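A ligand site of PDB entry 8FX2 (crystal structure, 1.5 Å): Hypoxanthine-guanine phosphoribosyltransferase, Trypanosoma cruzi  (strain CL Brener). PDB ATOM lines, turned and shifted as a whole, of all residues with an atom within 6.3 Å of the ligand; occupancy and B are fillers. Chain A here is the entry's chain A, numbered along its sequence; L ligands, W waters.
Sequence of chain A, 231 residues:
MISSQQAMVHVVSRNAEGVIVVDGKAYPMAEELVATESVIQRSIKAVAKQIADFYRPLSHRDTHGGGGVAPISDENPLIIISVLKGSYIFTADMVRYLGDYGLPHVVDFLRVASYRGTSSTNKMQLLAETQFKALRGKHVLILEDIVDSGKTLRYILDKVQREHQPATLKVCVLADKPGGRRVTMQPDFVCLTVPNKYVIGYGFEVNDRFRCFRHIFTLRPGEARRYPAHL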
ATOM      1  N   VAL A  83      30.772   0.028  11.562  1.00  0.00           N
ATOM      2  CA  VAL A  83      29.514  -0.344  10.858  1.00  0.00           C
ATOM      3  C   VAL A  83      28.359  -0.414  11.877  1.00  0.00           C
ATOM      4  O   VAL A  83      28.345  -1.293  12.720  1.00  0.00           O
ATOM      5  CB  VAL A  83      29.709  -1.662  10.084  1.00  0.00           C
ATOM      6  CG1 VAL A  83      28.435  -2.055   9.321  1.00  0.00           C
ATOM      7  CG2 VAL A  83      30.915  -1.572   9.123  1.00  0.00           C
ATOM      8  N   GLY A  86      25.315  -2.801  14.899  1.00  0.00           N
ATOM      9  CA  GLY A  86      25.894  -3.899  15.691  1.00  0.00           C
ATOM     10  C   GLY A  86      27.263  -3.674  16.257  1.00  0.00           C
ATOM     11  O   GLY A  86      27.596  -4.296  17.248  1.00  0.00           O
ATOM     12  N   MET A 124      22.089  -5.656  -1.080  1.00  0.00           N
ATOM     13  CA  MET A 124      22.587  -4.663  -0.076  1.00  0.00           C
ATOM     14  C   MET A 124      22.310  -3.214  -0.523  1.00  0.00           C
ATOM     15  O   MET A 124      22.300  -2.963  -1.708  1.00  0.00           O
ATOM     16  CB  MET A 124      24.091  -4.824   0.178  1.00  0.00           C
ATOM     17  CG  MET A 124      24.522  -6.194   0.711  1.00  0.00           C
ATOM     18  SD  MET A 124      23.883  -6.547   2.354  1.00  0.00           S
ATOM     19  CE  MET A 124      24.430  -5.112   3.275  1.00  0.00           C
ATOM     20  N   GLU A 144      33.665  -4.122  12.276  1.00  0.00           N
ATOM     21  CA  GLU A 144      32.356  -4.773  12.017  1.00  0.00           C
ATOM     22  C   GLU A 144      32.067  -5.803  13.120  1.00  0.00           C
ATOM     23  O   GLU A 144      33.002  -6.304  13.703  1.00  0.00           O
ATOM     24  CB  GLU A 144      32.378  -5.399  10.613  1.00  0.00           C
ATOM     25  CG  GLU A 144      31.151  -6.224  10.220  1.00  0.00           C
ATOM     26  CD  GLU A 144      29.831  -5.452  10.144  1.00  0.00           C
ATOM     27  OE1 GLU A 144      29.135  -5.543   9.121  1.00  0.00           O
ATOM     28  OE2 GLU A 144      29.474  -4.812  11.121  1.00  0.00           O
ATOM     29  N   ASP A 145      30.802  -6.100  13.383  1.00  0.00           N
ATOM     30  CA  ASP A 145      30.405  -7.014  14.474  1.00  0.00           C
ATOM     31  C   ASP A 145      30.732  -8.481  14.115  1.00  0.00           C
ATOM     32  O   ASP A 145      31.334  -9.176  14.919  1.00  0.00           O
ATOM     33  CB  ASP A 145      28.903  -6.832  14.803  1.00  0.00           C
ATOM     34  CG  ASP A 145      27.938  -6.977  13.643  1.00  0.00           C
ATOM     35  OD1 ASP A 145      28.363  -7.211  12.531  1.00  0.00           O
ATOM     36  OD2 ASP A 145      26.745  -6.827  13.865  1.00  0.00           O
ATOM     37  N   ILE A 146      30.305  -8.920  12.941  1.00  0.00           N
ATOM     38  CA  ILE A 146      30.489 -10.343  12.566  1.00  0.00           C
ATOM     39  C   ILE A 146      30.595 -10.529  11.065  1.00  0.00           C
ATOM     40  O   ILE A 146      29.969  -9.760  10.341  1.00  0.00           O
ATOM     41  CB  ILE A 146      29.344 -11.233  13.135  1.00  0.00           C
ATOM     42  CG1 ILE A 146      29.590 -12.740  12.941  1.00  0.00           C
ATOM     43  CG2 ILE A 146      27.979 -10.817  12.579  1.00  0.00           C
ATOM     44  CD1 ILE A 146      28.737 -13.631  13.866  1.00  0.00           C
ATOM     45  N   VAL A 147      31.417 -11.485  10.645  1.00  0.00           N
ATOM     46  CA  VAL A 147      31.453 -11.936   9.243  1.00  0.00           C
ATOM     47  C   VAL A 147      30.748 -13.297   9.292  1.00  0.00           C
ATOM     48  O   VAL A 147      31.182 -14.139  10.063  1.00  0.00           O
ATOM     49  CB  VAL A 147      32.878 -12.006   8.649  1.00  0.00           C
ATOM     50  CG1 VAL A 147      33.823 -12.926   9.438  1.00  0.00           C
ATOM     51  CG2 VAL A 147      32.830 -12.391   7.170  1.00  0.00           C
ATOM     52  N   ASP A 148      29.692 -13.477   8.524  1.00  0.00           N
ATOM     53  CA  ASP A 148      28.887 -14.722   8.484  1.00  0.00           C
ATOM     54  C   ASP A 148      28.942 -15.207   7.017  1.00  0.00           C
ATOM     55  O   ASP A 148      29.904 -15.875   6.685  1.00  0.00           O
ATOM     56  CB  ASP A 148      27.511 -14.441   9.104  1.00  0.00           C
ATOM     57  CG  ASP A 148      26.637 -15.676   9.296  1.00  0.00           C
ATOM     58  OD1 ASP A 148      26.887 -16.658   8.639  1.00  0.00           O
ATOM     59  OD2 ASP A 148      25.704 -15.620  10.094  1.00  0.00           O
ATOM     60  N   SER A 149      28.006 -14.824   6.160  1.00  0.00           N
ATOM     61  CA  SER A 149      28.046 -15.150   4.707  1.00  0.00           C
ATOM     62  C   SER A 149      29.203 -14.410   4.032  1.00  0.00           C
ATOM     63  O   SER A 149      29.706 -14.921   3.051  1.00  0.00           O
ATOM     64  CB  SER A 149      26.754 -14.837   3.971  1.00  0.00           C
ATOM     65  OG  SER A 149      26.552 -13.457   3.735  1.00  0.00           O
ATOM     66  N   GLY A 150      29.527 -13.217   4.517  1.00  0.00           N
ATOM     67  CA  GLY A 150      30.584 -12.362   3.936  1.00  0.00           C
ATOM     68  C   GLY A 150      30.032 -11.333   2.965  1.00  0.00           C
ATOM     69  O   GLY A 150      30.792 -10.516   2.495  1.00  0.00           O
ATOM     70  N   LYS A 151      28.745 -11.365   2.687  1.00  0.00           N
ATOM     71  CA  LYS A 151      28.153 -10.499   1.629  1.00  0.00           C
ATOM     72  C   LYS A 151      28.118  -9.042   2.096  1.00  0.00           C
ATOM     73  O   LYS A 151      28.362  -8.160   1.288  1.00  0.00           O
ATOM     74  CB  LYS A 151      26.768 -11.024   1.239  1.00  0.00           C
ATOM     75  CG  LYS A 151      26.762 -12.428   0.626  1.00  0.00           C
ATOM     76  CD  LYS A 151      25.429 -12.820  -0.075  1.00  0.00           C
ATOM     77  CE  LYS A 151      25.484 -12.607  -1.593  1.00  0.00           C
ATOM     78  NZ  LYS A 151      24.180 -12.922  -2.267  1.00  0.00           N
ATOM     79  N   THR A 152      27.810  -8.818   3.366  1.00  0.00           N
ATOM     80  CA  THR A 152      27.732  -7.432   3.891  1.00  0.00           C
ATOM     81  C   THR A 152      29.115  -6.771   3.742  1.00  0.00           C
ATOM     82  O   THR A 152      29.182  -5.668   3.231  1.00  0.00           O
ATOM     83  CB  THR A 152      27.197  -7.364   5.339  1.00  0.00           C
ATOM     84  OG1 THR A 152      25.893  -7.962   5.351  1.00  0.00           O
ATOM     85  CG2 THR A 152      27.153  -5.955   5.880  1.00  0.00           C
ATOM     86  N   LEU A 153      30.179  -7.429   4.165  1.00  0.00           N
ATOM     87  CA  LEU A 153      31.541  -6.811   4.148  1.00  0.00           C
ATOM     88  C   LEU A 153      32.062  -6.694   2.702  1.00  0.00           C
ATOM     89  O   LEU A 153      32.732  -5.750   2.412  1.00  0.00           O
ATOM     90  CB  LEU A 153      32.516  -7.584   5.036  1.00  0.00           C
ATOM     91  CG  LEU A 153      32.504  -7.245   6.533  1.00  0.00           C
ATOM     92  CD1 LEU A 153      33.239  -8.321   7.344  1.00  0.00           C
ATOM     93  CD2 LEU A 153      33.144  -5.868   6.773  1.00  0.00           C
ATOM     94  N   LYS A 177      32.128 -16.234  12.062  1.00  0.00           N
ATOM     95  CA  LYS A 177      31.317 -17.474  12.015  1.00  0.00           C
ATOM     96  C   LYS A 177      31.835 -18.214  10.775  1.00  0.00           C
ATOM     97  O   LYS A 177      31.272 -18.027   9.714  1.00  0.00           O
ATOM     98  CB  LYS A 177      29.816 -17.215  11.936  1.00  0.00           C
ATOM     99  CG  LYS A 177      28.943 -18.460  12.078  1.00  0.00           C
ATOM    100  CD  LYS A 177      27.440 -18.189  11.851  1.00  0.00           C
ATOM    101  CE  LYS A 177      26.886 -17.075  12.733  1.00  0.00           C
ATOM    102  NZ  LYS A 177      25.402 -16.935  12.578  1.00  0.00           N
ATOM    103  N   GLY A 180      29.488 -20.020   8.052  1.00  0.00           N
ATOM    104  CA  GLY A 180      28.451 -19.250   7.338  1.00  0.00           C
ATOM    105  C   GLY A 180      28.866 -18.739   5.972  1.00  0.00           C
ATOM    106  O   GLY A 180      28.003 -18.343   5.238  1.00  0.00           O
ATOM    107  N   VAL A 194      32.956 -17.916  16.515  1.00  0.00           N
ATOM    108  CA  VAL A 194      31.652 -18.341  17.081  1.00  0.00           C
ATOM    109  C   VAL A 194      31.177 -19.594  16.349  1.00  0.00           C
ATOM    110  O   VAL A 194      31.614 -19.836  15.237  1.00  0.00           O
ATOM    111  CB  VAL A 194      30.599 -17.205  16.987  1.00  0.00           C
ATOM    112  CG1 VAL A 194      31.059 -15.984  17.796  1.00  0.00           C
ATOM    113  CG2 VAL A 194      30.256 -16.818  15.552  1.00  0.00           C
ATOM    114  N   LYS A 197      25.832 -20.788  14.421  1.00  0.00           N
ATOM    115  CA  LYS A 197      24.501 -20.627  15.030  1.00  0.00           C
ATOM    116  C   LYS A 197      24.240 -19.127  15.117  1.00  0.00           C
ATOM    117  O   LYS A 197      25.190 -18.378  15.052  1.00  0.00           O
ATOM    118  CB  LYS A 197      24.494 -21.179  16.461  1.00  0.00           C
ATOM    119  CG  LYS A 197      24.864 -22.653  16.648  1.00  0.00           C
ATOM    120  CD  LYS A 197      23.725 -23.622  16.321  1.00  0.00           C
ATOM    121  CE  LYS A 197      24.014 -25.064  16.720  1.00  0.00           C
ATOM    122  NZ  LYS A 197      22.788 -25.926  16.658  1.00  0.00           N
ATOM    123  N   TYR A 198      23.000 -18.730  15.321  1.00  0.00           N
ATOM    124  CA  TYR A 198      22.654 -17.310  15.480  1.00  0.00           C
ATOM    125  C   TYR A 198      23.104 -16.841  16.868  1.00  0.00           C
ATOM    126  O   TYR A 198      22.659 -17.401  17.841  1.00  0.00           O
ATOM    127  CB  TYR A 198      21.163 -17.048  15.253  1.00  0.00           C
ATOM    128  CG  TYR A 198      20.838 -15.584  15.109  1.00  0.00           C
ATOM    129  CD1 TYR A 198      20.968 -14.962  13.883  1.00  0.00           C
ATOM    130  CD2 TYR A 198      20.498 -14.815  16.200  1.00  0.00           C
ATOM    131  CE1 TYR A 198      20.694 -13.610  13.728  1.00  0.00           C
ATOM    132  CE2 TYR A 198      20.218 -13.460  16.067  1.00  0.00           C
ATOM    133  CZ  TYR A 198      20.313 -12.860  14.824  1.00  0.00           C
ATOM    134  OH  TYR A 198      20.056 -11.531  14.640  1.00  0.00           O
ATOM    135  N   VAL A 199      24.003 -15.864  16.919  1.00  0.00           N
ATOM    136  CA  VAL A 199      24.554 -15.363  18.205  1.00  0.00           C
ATOM    137  C   VAL A 199      23.852 -14.075  18.659  1.00  0.00           C
ATOM    138  O   VAL A 199      23.360 -13.337  17.852  1.00  0.00           O
ATOM    139  CB  VAL A 199      26.089 -15.190  18.135  1.00  0.00           C
ATOM    140  CG1 VAL A 199      26.775 -16.552  18.017  1.00  0.00           C
ATOM    141  CG2 VAL A 199      26.562 -14.231  17.027  1.00  0.00           C
ATOM    142  N   ILE A 200      23.780 -13.875  19.955  1.00  0.00           N
ATOM    143  CA  ILE A 200      23.112 -12.698  20.568  1.00  0.00           C
ATOM    144  C   ILE A 200      24.003 -12.186  21.694  1.00  0.00           C
ATOM    145  O   ILE A 200      24.803 -12.942  22.203  1.00  0.00           O
ATOM    146  CB  ILE A 200      21.707 -13.045  21.079  1.00  0.00           C
ATOM    147  CG1 ILE A 200      21.735 -14.180  22.122  1.00  0.00           C
ATOM    148  CG2 ILE A 200      20.751 -13.358  19.918  1.00  0.00           C
ATOM    149  CD1 ILE A 200      20.474 -14.237  23.005  1.00  0.00           C
ATOM    150  N   PHE A 204      24.995  -8.011  19.368  1.00  0.00           N
ATOM    151  CA  PHE A 204      24.223  -8.938  18.508  1.00  0.00           C
ATOM    152  C   PHE A 204      22.773  -8.903  18.973  1.00  0.00           C
ATOM    153  O   PHE A 204      22.553  -9.048  20.163  1.00  0.00           O
ATOM    154  CB  PHE A 204      24.836 -10.340  18.478  1.00  0.00           C
ATOM    155  CG  PHE A 204      26.231 -10.391  17.920  1.00  0.00           C
ATOM    156  CD1 PHE A 204      26.481  -9.963  16.630  1.00  0.00           C
ATOM    157  CD2 PHE A 204      27.300 -10.841  18.685  1.00  0.00           C
ATOM    158  CE1 PHE A 204      27.759  -9.994  16.105  1.00  0.00           C
ATOM    159  CE2 PHE A 204      28.585 -10.887  18.159  1.00  0.00           C
ATOM    160  CZ  PHE A 204      28.811 -10.456  16.876  1.00  0.00           C
ATOM    161  N   GLU A 205      21.835  -8.798  18.038  1.00  0.00           N
ATOM    162  CA  GLU A 205      20.432  -8.552  18.372  1.00  0.00           C
ATOM    163  C   GLU A 205      19.402  -9.525  17.857  1.00  0.00           C
ATOM    164  O   GLU A 205      19.746 -10.340  17.034  1.00  0.00           O
ATOM    165  CB  GLU A 205      19.993  -7.240  17.680  1.00  0.00           C
ATOM    166  CG  GLU A 205      20.201  -7.238  16.149  1.00  0.00           C
ATOM    167  CD  GLU A 205      19.286  -6.372  15.288  1.00  0.00           C
ATOM    168  OE1 GLU A 205      18.346  -5.770  15.801  1.00  0.00           O
ATOM    169  OE2 GLU A 205      19.527  -6.304  14.073  1.00  0.00           O
ATOM    170  N   ARG A 211      21.204  -6.678  22.777  1.00  0.00           N
ATOM    171  CA  ARG A 211      22.495  -6.022  22.426  1.00  0.00           C
ATOM    172  C   ARG A 211      23.258  -5.639  23.713  1.00  0.00           C
ATOM    173  O   ARG A 211      24.467  -5.626  23.669  1.00  0.00           O
ATOM    174  CB  ARG A 211      22.324  -4.738  21.620  1.00  0.00           C
ATOM    175  CG  ARG A 211      21.689  -4.897  20.235  1.00  0.00           C
ATOM    176  CD  ARG A 211      21.969  -3.642  19.397  1.00  0.00           C
ATOM    177  NE  ARG A 211      21.172  -3.497  18.178  1.00  0.00           N
ATOM    178  CZ  ARG A 211      21.534  -3.887  16.944  1.00  0.00           C
ATOM    179  NH1 ARG A 211      22.685  -4.516  16.733  1.00  0.00           N
ATOM    180  NH2 ARG A 211      20.717  -3.653  15.913  1.00  0.00           N
HETATM  181  P1  LIG L   1      26.787 -11.461   6.488  1.00  0.00           P
HETATM  182  O1  LIG L   1      26.458 -10.653   5.272  1.00  0.00           O
HETATM  183  O2  LIG L   1      26.007 -12.780   6.352  1.00  0.00           O
HETATM  184  O3  LIG L   1      28.256 -11.659   6.746  1.00  0.00           O
HETATM  185  O4  LIG L   1      26.106 -10.874   7.886  1.00  0.00           O
HETATM  186  C1  LIG L   1      26.533  -9.660   8.431  1.00  0.00           C
HETATM  187  C2  LIG L   1      25.347  -8.990   9.125  1.00  0.00           C
HETATM  188  N1  LIG L   1      24.255  -9.707   9.336  1.00  0.00           N
HETATM  189  C3  LIG L   1      25.976  -8.600  10.663  1.00  0.00           C
HETATM  190  O5  LIG L   1      26.554  -7.281  10.601  1.00  0.00           O
HETATM  191  C4  LIG L   1      25.039  -8.658  11.533  1.00  0.00           C
HETATM  192  O6  LIG L   1      24.338  -7.378  11.739  1.00  0.00           O
HETATM  193  C5  LIG L   1      24.063  -9.723  10.888  1.00  0.00           C
HETATM  194  C6  LIG L   1      24.323 -11.027  11.384  1.00  0.00           C
HETATM  195  C7  LIG L   1      24.896 -12.093  10.703  1.00  0.00           C
HETATM  196  N2  LIG L   1      24.966 -13.157  11.532  1.00  0.00           N
HETATM  197  C8  LIG L   1      24.061 -11.495  12.671  1.00  0.00           C
HETATM  198  O7  LIG L   1      24.650 -14.744  14.151  1.00  0.00           O
HETATM  199  C9  LIG L   1      24.337 -13.576  14.022  1.00  0.00           C
HETATM  200  N3  LIG L   1      23.741 -12.893  15.116  1.00  0.00           N
HETATM  201  C10 LIG L   1      23.321 -11.539  15.049  1.00  0.00           C
HETATM  202  N4  LIG L   1      23.481 -10.804  13.843  1.00  0.00           N
HETATM  203  C11 LIG L   1      24.471 -12.816  12.739  1.00  0.00           C
HETATM  204  O   HOH W   1      24.803  -4.577  12.263  1.00  0.00           O
HETATM  205  O   HOH W   2      22.972  -5.690  14.170  1.00  0.00           O
HETATM  206  O   HOH W   3      23.871 -10.791   4.308  1.00  0.00           O
HETATM  207  O   HOH W   4      23.616 -13.839   6.766  1.00  0.00           O
HETATM  208  O   HOH W   5      21.322  -7.571  12.517  1.00  0.00           O
HETATM  209  O   HOH W   6      26.353  -4.845   9.248  1.00  0.00           O
HETATM  210  O   HOH W   7      29.459  -8.122   8.176  1.00  0.00           O
HETATM  211  O   HOH W   8      23.007  -8.434  15.255  1.00  0.00           O
HETATM  212  O   HOH W   9      29.991  -9.697   6.117  1.00  0.00           O
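Water W6 bridges O5 of the ligand (2.8 Å) and OE1 of Glu 144 (2.9 Å).
Water W8 lies within hydrogen-bond range of a nitrogen (N4) of the ligand and the backbone NH (N) of Glu 205.
Water W1 lies within hydrogen-bond range of an oxygen (O6) of the ligand (2.9 Å), the backbone NH (N) of Gly 86 (3.2 Å) and the side-chain carboxylate (OD2) of Asp 145 (3.4 Å).
Water W5 bridges the side-chain carboxylate of Glu 205 and an oxygen (O6) of the ligand.
Water W2 lies within hydrogen-bond range of NH1 of Arg 211 (2.8 Å), O6 of the ligand (3.3 Å) and OE2 of Glu 205 (3.5 Å).
Water W7 bridges O of Ile 146 (2.8 Å) and OE1 of Glu 144 (2.8 Å).
Residues that only touch the ligand: Ile 146 (3.5 Å), Val 147 (3.9 Å), Lys 151 (3.5 Å), Lys 197 (3.8 Å), Tyr 198 (3.3 Å) and Phe 204 (3.9 Å).
Hydrophobic or aromatic side chains within 4 Å of the ligand: Ile 146, Tyr 198, Val 199 and Phe 204.
Within 4 Å of the ligand: Glu 144, Asp 145, Ile 146, Val 147, Asp 148, Ser 149, Gly 150, Lys 151, Thr 152, Lys 177, Lys 197, Tyr 198, Val 199 and Phe 204.
Along chain A the residues within 4 Å of the ligand span positions 144 to 204.
The nearest printed residue that does not touch the ligand is Glu 205 (4.3 Å).
OG of Ser 149 is in hydrogen-bond range of N of Lys 151 (3.2 Å).
The side-chain amino group (NZ) of Lys 177 is in salt-bridge range of the side-chain carboxylate (OD2) of Asp 148 (2.8 Å).
The side-chain amino group (NZ) of Lys 177 sits at hydrogen-bond distance from the backbone carbonyl oxygen (O) of Lys 197 (2.9 Å).
N of Lys 177 lies within hydrogen-bond range of O of Val 147, at 3.0 Å.
OH of Tyr 198 sits at hydrogen-bond distance from O of Glu 205.
The side-chain carboxylate (OD1) of Asp 145 sits at hydrogen-bond distance from an oxygen (O5) of the ligand (2.6 Å).
The backbone NH (N) of Thr 152 sits at hydrogen-bond distance from an oxygen (O1) of the ligand (3.0 Å).
OG1 of Thr 152 lies within hydrogen-bond range of O1 of the ligand, at 2.8 Å.
O2 of the ligand lies within hydrogen-bond range of N of Ser 149.
OG of Ser 149 sits at hydrogen-bond distance from O2 of the ligand (2.8 Å).
The backbone NH of Val 199 is in hydrogen-bond range of an oxygen (O7) of the ligand, at 3.1 Å.
The backbone carbonyl oxygen of Val 199 sits at hydrogen-bond distance from a nitrogen (N3) of the ligand (2.8 Å).
The side-chain amino group of Lys 177 sits at hydrogen-bond distance from an oxygen (O7) of the ligand (2.8 Å).
O3 of the ligand is in hydrogen-bond range of N of Asp 148, 2.9 Å away.
A nitrogen (N2) of the ligand lies within hydrogen-bond range of the side-chain carboxylate (OD2) of Asp 148 (2.9 Å).
An oxygen (O3) of the ligand sits at hydrogen-bond distance from the backbone NH (N) of Gly 150 (3.0 Å).
An oxygen (O5) of the ligand is in hydrogen-bond range of the side-chain carboxylate (OE1) of Glu 144, at 3.4 Å.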
